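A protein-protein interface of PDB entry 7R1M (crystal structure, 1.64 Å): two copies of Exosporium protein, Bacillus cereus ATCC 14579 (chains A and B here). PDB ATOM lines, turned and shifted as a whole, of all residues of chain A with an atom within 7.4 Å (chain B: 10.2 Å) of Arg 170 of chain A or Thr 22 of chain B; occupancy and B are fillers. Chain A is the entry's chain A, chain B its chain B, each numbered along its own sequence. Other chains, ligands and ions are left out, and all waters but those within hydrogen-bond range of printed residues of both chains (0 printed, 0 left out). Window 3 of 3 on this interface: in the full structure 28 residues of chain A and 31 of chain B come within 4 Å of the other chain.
Ala 75 of chain A touches none of the printed residues of chain B.
Of the printed residues of chain B, Ile 168 of chain A touches Pro 24 (3.6 Å).
Of the printed residues of chain B, Ser 169 of chain A touches Leu 23 (3.6 Å), Pro 24 (3.5 Å) and Phe 26 (3.9997 Å).
Of chain B, only Thr 22 and Leu 23 come within 4 Å of Arg 170 of chain A.
No residue of chain B comes within 4 Å of Pro 171 of chain A.
Of the printed residues of chain B, His 172 of chain A touches Leu 23, Phe 26, Pro 58 and Ile 60.
Printed residues of chain A within 4 Å of Thr 22 of chain B: Arg 170.
Printed residues of chain A within 4 Å of Leu 23 of chain B: Ser 169, Arg 170 and His 172.
Of the printed residues of chain A, Phe 26 of chain B touches Ile 77 (3.5 Å), Ser 169 (3.9997 Å) and His 172 (3.7 Å).
Asp 62 of chain B touches none of the printed residues of chain A.
The nearest printed residue of chain B that does not touch Arg 170 of chain A is Pro 24 of chain B (5.6 Å).
The nearest residue of chain A that does not touch Thr 22 of chain B is Ser 169 of chain A (5.9 Å).
The nearest printed residue of chain B that does not touch Ile 168 of chain A is Phe 26 of chain B (4.2 Å).
The backbone carbonyl oxygen of Ser 169 of chain A lies within hydrogen-bond range of the backbone NH of Ile 77 of chain A (2.8 Å).
The backbone carbonyl oxygen (O) of Leu 23 of chain B lies close to the side-chain amide nitrogen (ND2) of Asn 61 of chain B, 3.4 Å away.
The side-chain amide nitrogen of Gln 167 of chain A lies within hydrogen-bond range of the backbone carbonyl oxygen of Ser 169 of chain A (3.2 Å).
The backbone NH (N) of Phe 26 of chain B sits at hydrogen-bond distance from the backbone carbonyl oxygen (O) of Asn 61 of chain B, at 2.8 Å.
The side-chain amide nitrogen (ND2) of Asn 61 of chain B is in hydrogen-bond range of the backbone carbonyl oxygen (O) of Pro 24 of chain B (3.0 Å).
O of Ile 77 of chain A is in hydrogen-bond range of N of Ile 168 of chain A, at 2.8 Å.
Arg 170 of chain A touches Thr 22 of chain B, but with the chains exchanged Thr 22 of chain A does not touch Arg 170 of chain B (13.9 Å).
Of the 11 pairs that touch across the chains among the printed residues, none has its exchanged pair printed and touching as well.
Hydrophobic or aromatic side chains of chain A within 4 Å of the printed part of chain B: Ile 77 and His 172.
Of the 17 printed residues of chain B, 6 touch a printed residue of chain A.
Among the printed residues, 11 pairs touch across the chains.
CG1 of Ile 77 of chain A touches CZ of Phe 26 of chain B, at 3.5 Å.
Ile 168 of chain A touches Pro 24 of chain B (O to CG, 3.6 Å).
OG of Ser 169 of chain A touches CD2 of Leu 23 of chain B, 3.6 Å away.
Ser 169 of chain A touches Pro 24 of chain B (OG to CD, 3.5 Å).
Phe 26 of chain B touches Ser 169 of chain A.
Arg 170 of chain A touches Thr 22 of chain B (NH1 to O, 3.8 Å).
Arg 170 of chain A touches Leu 23 of chain B.
CA of His 172 of chain A touches CD1 of Leu 23 of chain B, 3.8 Å away.
His 172 of chain A touches Phe 26 of chain B (ND1 to CZ, 3.7 Å).
A ring nitrogen (NE2) of His 172 of chain A lies within hydrogen-bond range of the backbone carbonyl oxygen (O) of Pro 58 of chain B (3.2 Å).
The backbone carbonyl oxygen of Ile 60 of chain B is in hydrogen-bond range of a ring nitrogen (NE2) of His 172 of chain A (3.2 Å).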
ATOM      1  N   THR A  22      -2.663  -9.919  -3.850  1.00  0.00           N
ATOM      2  CA  THR A  22      -2.194  -8.495  -3.887  1.00  0.00           C
ATOM      3  C   THR A  22      -0.678  -8.499  -4.143  1.00  0.00           C
ATOM      4  O   THR A  22       0.019  -9.428  -3.689  1.00  0.00           O
ATOM      5  CB  THR A  22      -2.633  -7.739  -2.621  1.00  0.00           C
ATOM      6  OG1 THR A  22      -2.605  -6.333  -2.876  1.00  0.00           O
ATOM      7  CG2 THR A  22      -1.791  -8.069  -1.404  1.00  0.00           C
ATOM      8  N   ARG A  74       3.579   1.936   1.414  1.00  0.00           N
ATOM      9  CA  ARG A  74       3.170   0.758   2.220  1.00  0.00           C
ATOM     10  C   ARG A  74       4.270   0.361   3.209  1.00  0.00           C
ATOM     11  O   ARG A  74       5.427   0.209   2.785  1.00  0.00           O
ATOM     12  CB  ARG A  74       2.857  -0.390   1.256  1.00  0.00           C
ATOM     13  CG  ARG A  74       2.217  -1.611   1.898  1.00  0.00           C
ATOM     14  CD  ARG A  74       2.254  -2.810   0.968  1.00  0.00           C
ATOM     15  NE  ARG A  74       1.641  -2.552  -0.325  1.00  0.00           N
ATOM     16  CZ  ARG A  74       1.570  -3.434  -1.311  1.00  0.00           C
ATOM     17  NH1 ARG A  74       0.990  -3.106  -2.452  1.00  0.00           N
ATOM     18  NH2 ARG A  74       2.078  -4.643  -1.158  1.00  0.00           N
ATOM     19  N   ALA A  75       3.905   0.179   4.479  1.00  0.00           N
ATOM     20  CA  ALA A  75       4.888  -0.267   5.492  1.00  0.00           C
ATOM     21  C   ALA A  75       5.314  -1.703   5.184  1.00  0.00           C
ATOM     22  O   ALA A  75       4.448  -2.506   4.790  1.00  0.00           O
ATOM     23  CB  ALA A  75       4.289  -0.167   6.870  1.00  0.00           C
ATOM     24  N   GLY A  76       6.604  -2.001   5.336  1.00  0.00           N
ATOM     25  CA  GLY A  76       7.078  -3.380   5.132  1.00  0.00           C
ATOM     26  C   GLY A  76       8.591  -3.461   5.150  1.00  0.00           C
ATOM     27  O   GLY A  76       9.230  -2.425   5.392  1.00  0.00           O
ATOM     28  N   ILE A  77       9.138  -4.650   4.897  1.00  0.00           N
ATOM     29  CA  ILE A  77      10.617  -4.809   4.802  1.00  0.00           C
ATOM     30  C   ILE A  77      10.959  -4.676   3.320  1.00  0.00           C
ATOM     31  O   ILE A  77      10.277  -5.322   2.508  1.00  0.00           O
ATOM     32  CB  ILE A  77      11.060  -6.165   5.385  1.00  0.00           C
ATOM     33  CG1 ILE A  77      10.579  -6.332   6.828  1.00  0.00           C
ATOM     34  CG2 ILE A  77      12.567  -6.340   5.268  1.00  0.00           C
ATOM     35  CD1 ILE A  77      11.232  -5.382   7.801  1.00  0.00           C
ATOM     36  N   GLN A 167       9.527  -4.735  -2.222  1.00  0.00           N
ATOM     37  CA  GLN A 167       9.086  -5.142  -0.861  1.00  0.00           C
ATOM     38  C   GLN A 167       9.348  -6.631  -0.636  1.00  0.00           C
ATOM     39  O   GLN A 167       8.753  -7.445  -1.362  1.00  0.00           O
ATOM     40  CB  GLN A 167       7.593  -4.860  -0.676  1.00  0.00           C
ATOM     41  CG  GLN A 167       7.087  -5.146   0.729  1.00  0.00           C
ATOM     42  CD  GLN A 167       5.587  -5.019   0.819  1.00  0.00           C
ATOM     43  OE1 GLN A 167       4.903  -4.815  -0.180  1.00  0.00           O
ATOM     44  NE2 GLN A 167       5.063  -5.142   2.027  1.00  0.00           N
ATOM     45  N   ILE A 168      10.255  -6.960   0.285  1.00  0.00           N
ATOM     46  CA  ILE A 168      10.512  -8.383   0.652  1.00  0.00           C
ATOM     47  C   ILE A 168       9.320  -8.945   1.433  1.00  0.00           C
ATOM     48  O   ILE A 168       8.892 -10.069   1.123  1.00  0.00           O
ATOM     49  CB  ILE A 168      11.819  -8.485   1.465  1.00  0.00           C
ATOM     50  CG1 ILE A 168      13.018  -7.983   0.658  1.00  0.00           C
ATOM     51  CG2 ILE A 168      12.043  -9.897   1.979  1.00  0.00           C
ATOM     52  CD1 ILE A 168      13.280  -8.783  -0.595  1.00  0.00           C
ATOM     53  N   SER A 169       8.780  -8.178   2.384  1.00  0.00           N
ATOM     54  CA  SER A 169       7.718  -8.737   3.260  1.00  0.00           C
ATOM     55  C   SER A 169       6.870  -7.642   3.907  1.00  0.00           C
ATOM     56  O   SER A 169       7.297  -6.478   3.887  1.00  0.00           O
ATOM     57  CB  SER A 169       8.346  -9.592   4.331  1.00  0.00           C
ATOM     58  OG  SER A 169       7.376 -10.063   5.252  1.00  0.00           O
ATOM     59  N   ARG A 170       5.717  -8.038   4.453  1.00  0.00           N
ATOM     60  CA  ARG A 170       4.882  -7.080   5.214  1.00  0.00           C
ATOM     61  C   ARG A 170       5.542  -6.944   6.598  1.00  0.00           C
ATOM     62  O   ARG A 170       6.407  -7.791   6.895  1.00  0.00           O
ATOM     63  CB  ARG A 170       3.434  -7.580   5.270  1.00  0.00           C
ATOM     64  CG  ARG A 170       3.224  -8.806   6.145  1.00  0.00           C
ATOM     65  CD  ARG A 170       1.808  -9.344   6.068  1.00  0.00           C
ATOM     66  NE  ARG A 170       1.464  -9.805   4.731  1.00  0.00           N
ATOM     67  CZ  ARG A 170       1.607 -11.054   4.302  1.00  0.00           C
ATOM     68  NH1 ARG A 170       2.090 -11.984   5.111  1.00  0.00           N
ATOM     69  NH2 ARG A 170       1.267 -11.372   3.066  1.00  0.00           N
ATOM     70  N   PRO A 171       5.221  -5.950   7.466  1.00  0.00           N
ATOM     71  CA  PRO A 171       5.953  -5.800   8.732  1.00  0.00           C
ATOM     72  C   PRO A 171       5.946  -7.102   9.547  1.00  0.00           C
ATOM     73  O   PRO A 171       4.897  -7.704   9.670  1.00  0.00           O
ATOM     74  CB  PRO A 171       5.175  -4.698   9.462  1.00  0.00           C
ATOM     75  CG  PRO A 171       4.532  -3.900   8.351  1.00  0.00           C
ATOM     76  CD  PRO A 171       4.192  -4.923   7.288  1.00  0.00           C
ATOM     77  N   HIS A 172       7.107  -7.503  10.078  1.00  0.00           N
ATOM     78  CA  HIS A 172       7.221  -8.808  10.787  1.00  0.00           C
ATOM     79  C   HIS A 172       7.013  -8.663  12.299  1.00  0.00           C
ATOM     80  O   HIS A 172       7.039  -9.695  12.996  1.00  0.00           O
ATOM     81  CB  HIS A 172       8.564  -9.477  10.457  1.00  0.00           C
ATOM     82  CG  HIS A 172       9.754  -8.761  11.004  1.00  0.00           C
ATOM     83  ND1 HIS A 172      10.226  -7.584  10.461  1.00  0.00           N
ATOM     84  CD2 HIS A 172      10.575  -9.058  12.035  1.00  0.00           C
ATOM     85  CE1 HIS A 172      11.282  -7.182  11.136  1.00  0.00           C
ATOM     86  NE2 HIS A 172      11.517  -8.069  12.107  1.00  0.00           N
ATOM     87  N   HIS A 173       6.824  -7.436  12.785  1.00  0.00           N
ATOM     88  CA  HIS A 173       6.630  -7.204  14.240  1.00  0.00           C
ATOM     89  C   HIS A 173       5.432  -6.271  14.430  1.00  0.00           C
ATOM     90  O   HIS A 173       5.001  -6.083  15.586  1.00  0.00           O
ATOM     91  CB  HIS A 173       7.923  -6.653  14.859  1.00  0.00           C
ATOM     92  CG  HIS A 173       7.873  -6.496  16.341  1.00  0.00           C
ATOM     93  ND1 HIS A 173       7.846  -7.578  17.199  1.00  0.00           N
ATOM     94  CD2 HIS A 173       7.845  -5.393  17.121  1.00  0.00           C
ATOM     95  CE1 HIS A 173       7.802  -7.149  18.443  1.00  0.00           C
ATOM     96  NE2 HIS A 173       7.801  -5.811  18.422  1.00  0.00           N
ATOM     97  N   HIS A 174       4.896  -5.736  13.331  1.00  0.00           N
ATOM     98  CA  HIS A 174       3.788  -4.745  13.438  1.00  0.00           C
ATOM     99  C   HIS A 174       2.589  -5.156  12.573  1.00  0.00           C
ATOM    100  O   HIS A 174       2.806  -5.620  11.443  1.00  0.00           O
ATOM    101  CB  HIS A 174       4.308  -3.332  13.152  1.00  0.00           C
ATOM    102  CG  HIS A 174       5.259  -2.842  14.193  1.00  0.00           C
ATOM    103  ND1 HIS A 174       6.628  -2.945  14.050  1.00  0.00           N
ATOM    104  CD2 HIS A 174       5.044  -2.272  15.398  1.00  0.00           C
ATOM    105  CE1 HIS A 174       7.219  -2.443  15.115  1.00  0.00           C
ATOM    106  NE2 HIS A 174       6.268  -2.026  15.958  1.00  0.00           N
ATOM    107  N   HIS A 175       1.369  -5.008  13.099  1.00  0.00           N
ATOM    108  CA  HIS A 175       0.153  -5.388  12.331  1.00  0.00           C
ATOM    109  C   HIS A 175      -0.016  -4.511  11.080  1.00  0.00           C
ATOM    110  O   HIS A 175      -0.317  -5.077  10.012  1.00  0.00           O
ATOM    111  CB  HIS A 175      -1.082  -5.380  13.241  1.00  0.00           C
ATOM    112  CG  HIS A 175      -1.288  -4.094  13.968  1.00  0.00           C
ATOM    113  ND1 HIS A 175      -0.446  -3.673  14.980  1.00  0.00           N
ATOM    114  CD2 HIS A 175      -2.232  -3.136  13.837  1.00  0.00           C
ATOM    115  CE1 HIS A 175      -0.864  -2.513  15.442  1.00  0.00           C
ATOM    116  NE2 HIS A 175      -1.957  -2.162  14.758  1.00  0.00           N
ATOM    117  N   THR B  22       2.442 -16.909   5.602  1.00  0.00           N
ATOM    118  CA  THR B  22       3.571 -16.779   6.562  1.00  0.00           C
ATOM    119  C   THR B  22       4.504 -15.662   6.083  1.00  0.00           C
ATOM    120  O   THR B  22       4.249 -15.114   4.992  1.00  0.00           O
ATOM    121  CB  THR B  22       4.302 -18.115   6.740  1.00  0.00           C
ATOM    122  OG1 THR B  22       5.229 -17.992   7.819  1.00  0.00           O
ATOM    123  CG2 THR B  22       5.023 -18.569   5.488  1.00  0.00           C
ATOM    124  N   LEU B  23       5.536 -15.342   6.868  1.00  0.00           N
ATOM    125  CA  LEU B  23       6.461 -14.238   6.500  1.00  0.00           C
ATOM    126  C   LEU B  23       7.741 -14.814   5.870  1.00  0.00           C
ATOM    127  O   LEU B  23       8.259 -15.786   6.444  1.00  0.00           O
ATOM    128  CB  LEU B  23       6.778 -13.411   7.749  1.00  0.00           C
ATOM    129  CG  LEU B  23       5.581 -12.722   8.399  1.00  0.00           C
ATOM    130  CD1 LEU B  23       5.919 -12.266   9.809  1.00  0.00           C
ATOM    131  CD2 LEU B  23       5.112 -11.550   7.555  1.00  0.00           C
ATOM    132  N   PRO B  24       8.280 -14.296   4.732  1.00  0.00           N
ATOM    133  CA  PRO B  24       9.552 -14.795   4.206  1.00  0.00           C
ATOM    134  C   PRO B  24      10.672 -14.714   5.252  1.00  0.00           C
ATOM    135  O   PRO B  24      10.661 -13.792   6.042  1.00  0.00           O
ATOM    136  CB  PRO B  24       9.869 -13.824   3.061  1.00  0.00           C
ATOM    137  CG  PRO B  24       8.514 -13.326   2.616  1.00  0.00           C
ATOM    138  CD  PRO B  24       7.690 -13.261   3.884  1.00  0.00           C
ATOM    139  N   ALA B  25      11.604 -15.669   5.227  1.00  0.00           N
ATOM    140  CA  ALA B  25      12.745 -15.620   6.154  1.00  0.00           C
ATOM    141  C   ALA B  25      13.745 -14.600   5.617  1.00  0.00           C
ATOM    142  O   ALA B  25      13.887 -14.565   4.421  1.00  0.00           O
ATOM    143  CB  ALA B  25      13.363 -16.977   6.300  1.00  0.00           C
ATOM    144  N   PHE B  26      14.381 -13.820   6.492  1.00  0.00           N
ATOM    145  CA  PHE B  26      15.379 -12.819   6.017  1.00  0.00           C
ATOM    146  C   PHE B  26      16.263 -12.402   7.177  1.00  0.00           C
ATOM    147  O   PHE B  26      15.906 -12.651   8.342  1.00  0.00           O
ATOM    148  CB  PHE B  26      14.695 -11.622   5.332  1.00  0.00           C
ATOM    149  CG  PHE B  26      13.696 -10.870   6.183  1.00  0.00           C
ATOM    150  CD1 PHE B  26      14.117  -9.974   7.150  1.00  0.00           C
ATOM    151  CD2 PHE B  26      12.330 -11.083   6.027  1.00  0.00           C
ATOM    152  CE1 PHE B  26      13.194  -9.255   7.892  1.00  0.00           C
ATOM    153  CE2 PHE B  26      11.409 -10.372   6.782  1.00  0.00           C
ATOM    154  CZ  PHE B  26      11.844  -9.475   7.718  1.00  0.00           C
ATOM    155  N   VAL B  57      14.895  -1.066  14.344  1.00  0.00           N
ATOM    156  CA  VAL B  57      14.369  -2.401  14.715  1.00  0.00           C
ATOM    157  C   VAL B  57      15.176  -3.492  13.998  1.00  0.00           C
ATOM    158  O   VAL B  57      15.676  -3.234  12.923  1.00  0.00           O
ATOM    159  CB  VAL B  57      12.879  -2.483  14.363  1.00  0.00           C
ATOM    160  CG1 VAL B  57      12.656  -2.423  12.874  1.00  0.00           C
ATOM    161  CG2 VAL B  57      12.254  -3.736  14.926  1.00  0.00           C
ATOM    162  N   PRO B  58      15.334  -4.692  14.583  1.00  0.00           N
ATOM    163  CA  PRO B  58      16.071  -5.785  13.957  1.00  0.00           C
ATOM    164  C   PRO B  58      15.397  -6.281  12.674  1.00  0.00           C
ATOM    165  O   PRO B  58      14.261  -6.570  12.691  1.00  0.00           O
ATOM    166  CB  PRO B  58      16.069  -6.877  15.023  1.00  0.00           C
ATOM    167  CG  PRO B  58      15.840  -6.132  16.281  1.00  0.00           C
ATOM    168  CD  PRO B  58      14.856  -5.057  15.896  1.00  0.00           C
ATOM    169  N   VAL B  59      16.164  -6.322  11.595  1.00  0.00           N
ATOM    170  CA  VAL B  59      15.710  -6.773  10.260  1.00  0.00           C
ATOM    171  C   VAL B  59      16.094  -8.248  10.153  1.00  0.00           C
ATOM    172  O   VAL B  59      17.078  -8.632   9.455  1.00  0.00           O
ATOM    173  CB  VAL B  59      16.254  -5.861   9.138  1.00  0.00           C
ATOM    174  CG1 VAL B  59      15.855  -6.380   7.765  1.00  0.00           C
ATOM    175  CG2 VAL B  59      15.731  -4.437   9.281  1.00  0.00           C
ATOM    176  N   ILE B  60      15.330  -9.065  10.871  1.00  0.00           N
ATOM    177  CA  ILE B  60      15.625 -10.492  11.162  1.00  0.00           C
ATOM    178  C   ILE B  60      14.259 -11.143  11.270  1.00  0.00           C
ATOM    179  O   ILE B  60      13.468 -10.653  12.085  1.00  0.00           O
ATOM    180  CB  ILE B  60      16.437 -10.668  12.459  1.00  0.00           C
ATOM    181  CG1 ILE B  60      17.823 -10.022  12.380  1.00  0.00           C
ATOM    182  CG2 ILE B  60      16.533 -12.144  12.843  1.00  0.00           C
ATOM    183  CD1 ILE B  60      18.813 -10.819  11.550  1.00  0.00           C
ATOM    184  N   ASN B  61      13.972 -12.093  10.386  1.00  0.00           N
ATOM    185  CA  ASN B  61      12.792 -12.977  10.503  1.00  0.00           C
ATOM    186  C   ASN B  61      13.231 -14.406  10.211  1.00  0.00           C
ATOM    187  O   ASN B  61      13.623 -14.668   9.068  1.00  0.00           O
ATOM    188  CB  ASN B  61      11.661 -12.580   9.576  1.00  0.00           C
ATOM    189  CG  ASN B  61      10.407 -13.382   9.882  1.00  0.00           C
ATOM    190  OD1 ASN B  61      10.001 -13.448  11.036  1.00  0.00           O
ATOM    191  ND2 ASN B  61       9.856 -14.066   8.898  1.00  0.00           N
ATOM    192  N   ASP B  62      13.167 -15.276  11.218  1.00  0.00           N
ATOM    193  CA  ASP B  62      13.414 -16.744  11.099  1.00  0.00           C
ATOM    194  C   ASP B  62      14.796 -16.970  10.485  1.00  0.00           C
ATOM    195  O   ASP B  62      14.996 -17.921   9.706  1.00  0.00           O
ATOM    196  CB  ASP B  62      12.269 -17.413  10.338  1.00  0.00           C
ATOM    197  CG  ASP B  62      12.060 -18.871  10.741  1.00  0.00           C
ATOM    198  OD1 ASP B  62      12.379 -19.215  11.890  1.00  0.00           O
ATOM    199  OD2 ASP B  62      11.623 -19.660   9.884  1.00  0.00           O
ATOM    200  N   ARG B  74      15.057 -21.975   8.136  1.00  0.00           N
ATOM    201  CA  ARG B  74      13.973 -22.507   7.269  1.00  0.00           C
ATOM    202  C   ARG B  74      14.514 -22.891   5.887  1.00  0.00           C
ATOM    203  O   ARG B  74      15.166 -22.050   5.252  1.00  0.00           O
ATOM    204  CB  ARG B  74      12.878 -21.446   7.140  1.00  0.00           C
ATOM    205  CG  ARG B  74      11.652 -21.892   6.360  1.00  0.00           C
ATOM    206  CD  ARG B  74      10.806 -20.698   5.969  1.00  0.00           C
ATOM    207  NE  ARG B  74      10.440 -19.873   7.109  1.00  0.00           N
ATOM    208  CZ  ARG B  74       9.782 -18.725   7.020  1.00  0.00           C
ATOM    209  NH1 ARG B  74       9.418 -18.262   5.839  1.00  0.00           N
ATOM    210  NH2 ARG B  74       9.490 -18.042   8.110  1.00  0.00           N
ATOM    211  N   ALA B  75      14.208 -24.104   5.422  1.00  0.00           N
ATOM    212  CA  ALA B  75      14.639 -24.537   4.072  1.00  0.00           C
ATOM    213  C   ALA B  75      13.905 -23.719   3.006  1.00  0.00           C
ATOM    214  O   ALA B  75      12.699 -23.468   3.181  1.00  0.00           O
ATOM    215  CB  ALA B  75      14.387 -26.012   3.893  1.00  0.00           C
ATOM    216  N   GLN B 167      14.678 -14.902   1.756  1.00  0.00           N
ATOM    217  CA  GLN B 167      14.020 -16.046   1.077  1.00  0.00           C
ATOM    218  C   GLN B 167      13.194 -15.513  -0.093  1.00  0.00           C
ATOM    219  O   GLN B 167      12.447 -14.540   0.110  1.00  0.00           O
ATOM    220  CB  GLN B 167      13.119 -16.796   2.058  1.00  0.00           C
ATOM    221  CG  GLN B 167      12.579 -18.107   1.510  1.00  0.00           C
ATOM    222  CD  GLN B 167      11.630 -18.772   2.474  1.00  0.00           C
ATOM    223  OE1 GLN B 167      11.306 -18.229   3.527  1.00  0.00           O
ATOM    224  NE2 GLN B 167      11.175 -19.960   2.117  1.00  0.00           N
ATOM    225  N   SER B 169      11.620 -18.011  -2.208  1.00  0.00           N
ATOM    226  CA  SER B 169      10.636 -19.086  -2.497  1.00  0.00           C
ATOM    227  C   SER B 169      10.731 -20.243  -1.503  1.00  0.00           C
ATOM    228  O   SER B 169      11.800 -20.413  -0.894  1.00  0.00           O
ATOM    229  CB  SER B 169      10.825 -19.601  -3.901  1.00  0.00           C
ATOM    230  OG  SER B 169       9.906 -20.642  -4.194  1.00  0.00           O
ATOM    231  N   ARG B 170       9.638 -20.996  -1.378  1.00  0.00           N
ATOM    232  CA  ARG B 170       9.668 -22.222  -0.549  1.00  0.00           C
ATOM    233  C   ARG B 170      10.396 -23.277  -1.397  1.00  0.00           C
ATOM    234  O   ARG B 170      10.487 -23.047  -2.617  1.00  0.00           O
ATOM    235  CB  ARG B 170       8.234 -22.651  -0.225  1.00  0.00           C
ATOM    236  CG  ARG B 170       7.339 -21.511   0.237  1.00  0.00           C
ATOM    237  CD  ARG B 170       5.875 -21.904   0.285  1.00  0.00           C
ATOM    238  NE  ARG B 170       5.536 -22.687   1.466  1.00  0.00           N
ATOM    239  CZ  ARG B 170       5.003 -22.182   2.572  1.00  0.00           C
ATOM    240  NH1 ARG B 170       4.738 -20.889   2.648  1.00  0.00           N
ATOM    241  NH2 ARG B 170       4.729 -22.971   3.595  1.00  0.00           N
ATOM    242  N   PRO B 171      10.920 -24.417  -0.868  1.00  0.00           N
ATOM    243  CA  PRO B 171      11.635 -25.378  -1.716  1.00  0.00           C
ATOM    244  C   PRO B 171      10.838 -25.772  -2.968  1.00  0.00           C
ATOM    245  O   PRO B 171       9.750 -26.297  -2.824  1.00  0.00           O
ATOM    246  CB  PRO B 171      11.826 -26.602  -0.812  1.00  0.00           C
ATOM    247  CG  PRO B 171      11.899 -26.015   0.572  1.00  0.00           C
ATOM    248  CD  PRO B 171      10.900 -24.879   0.539  1.00  0.00           C
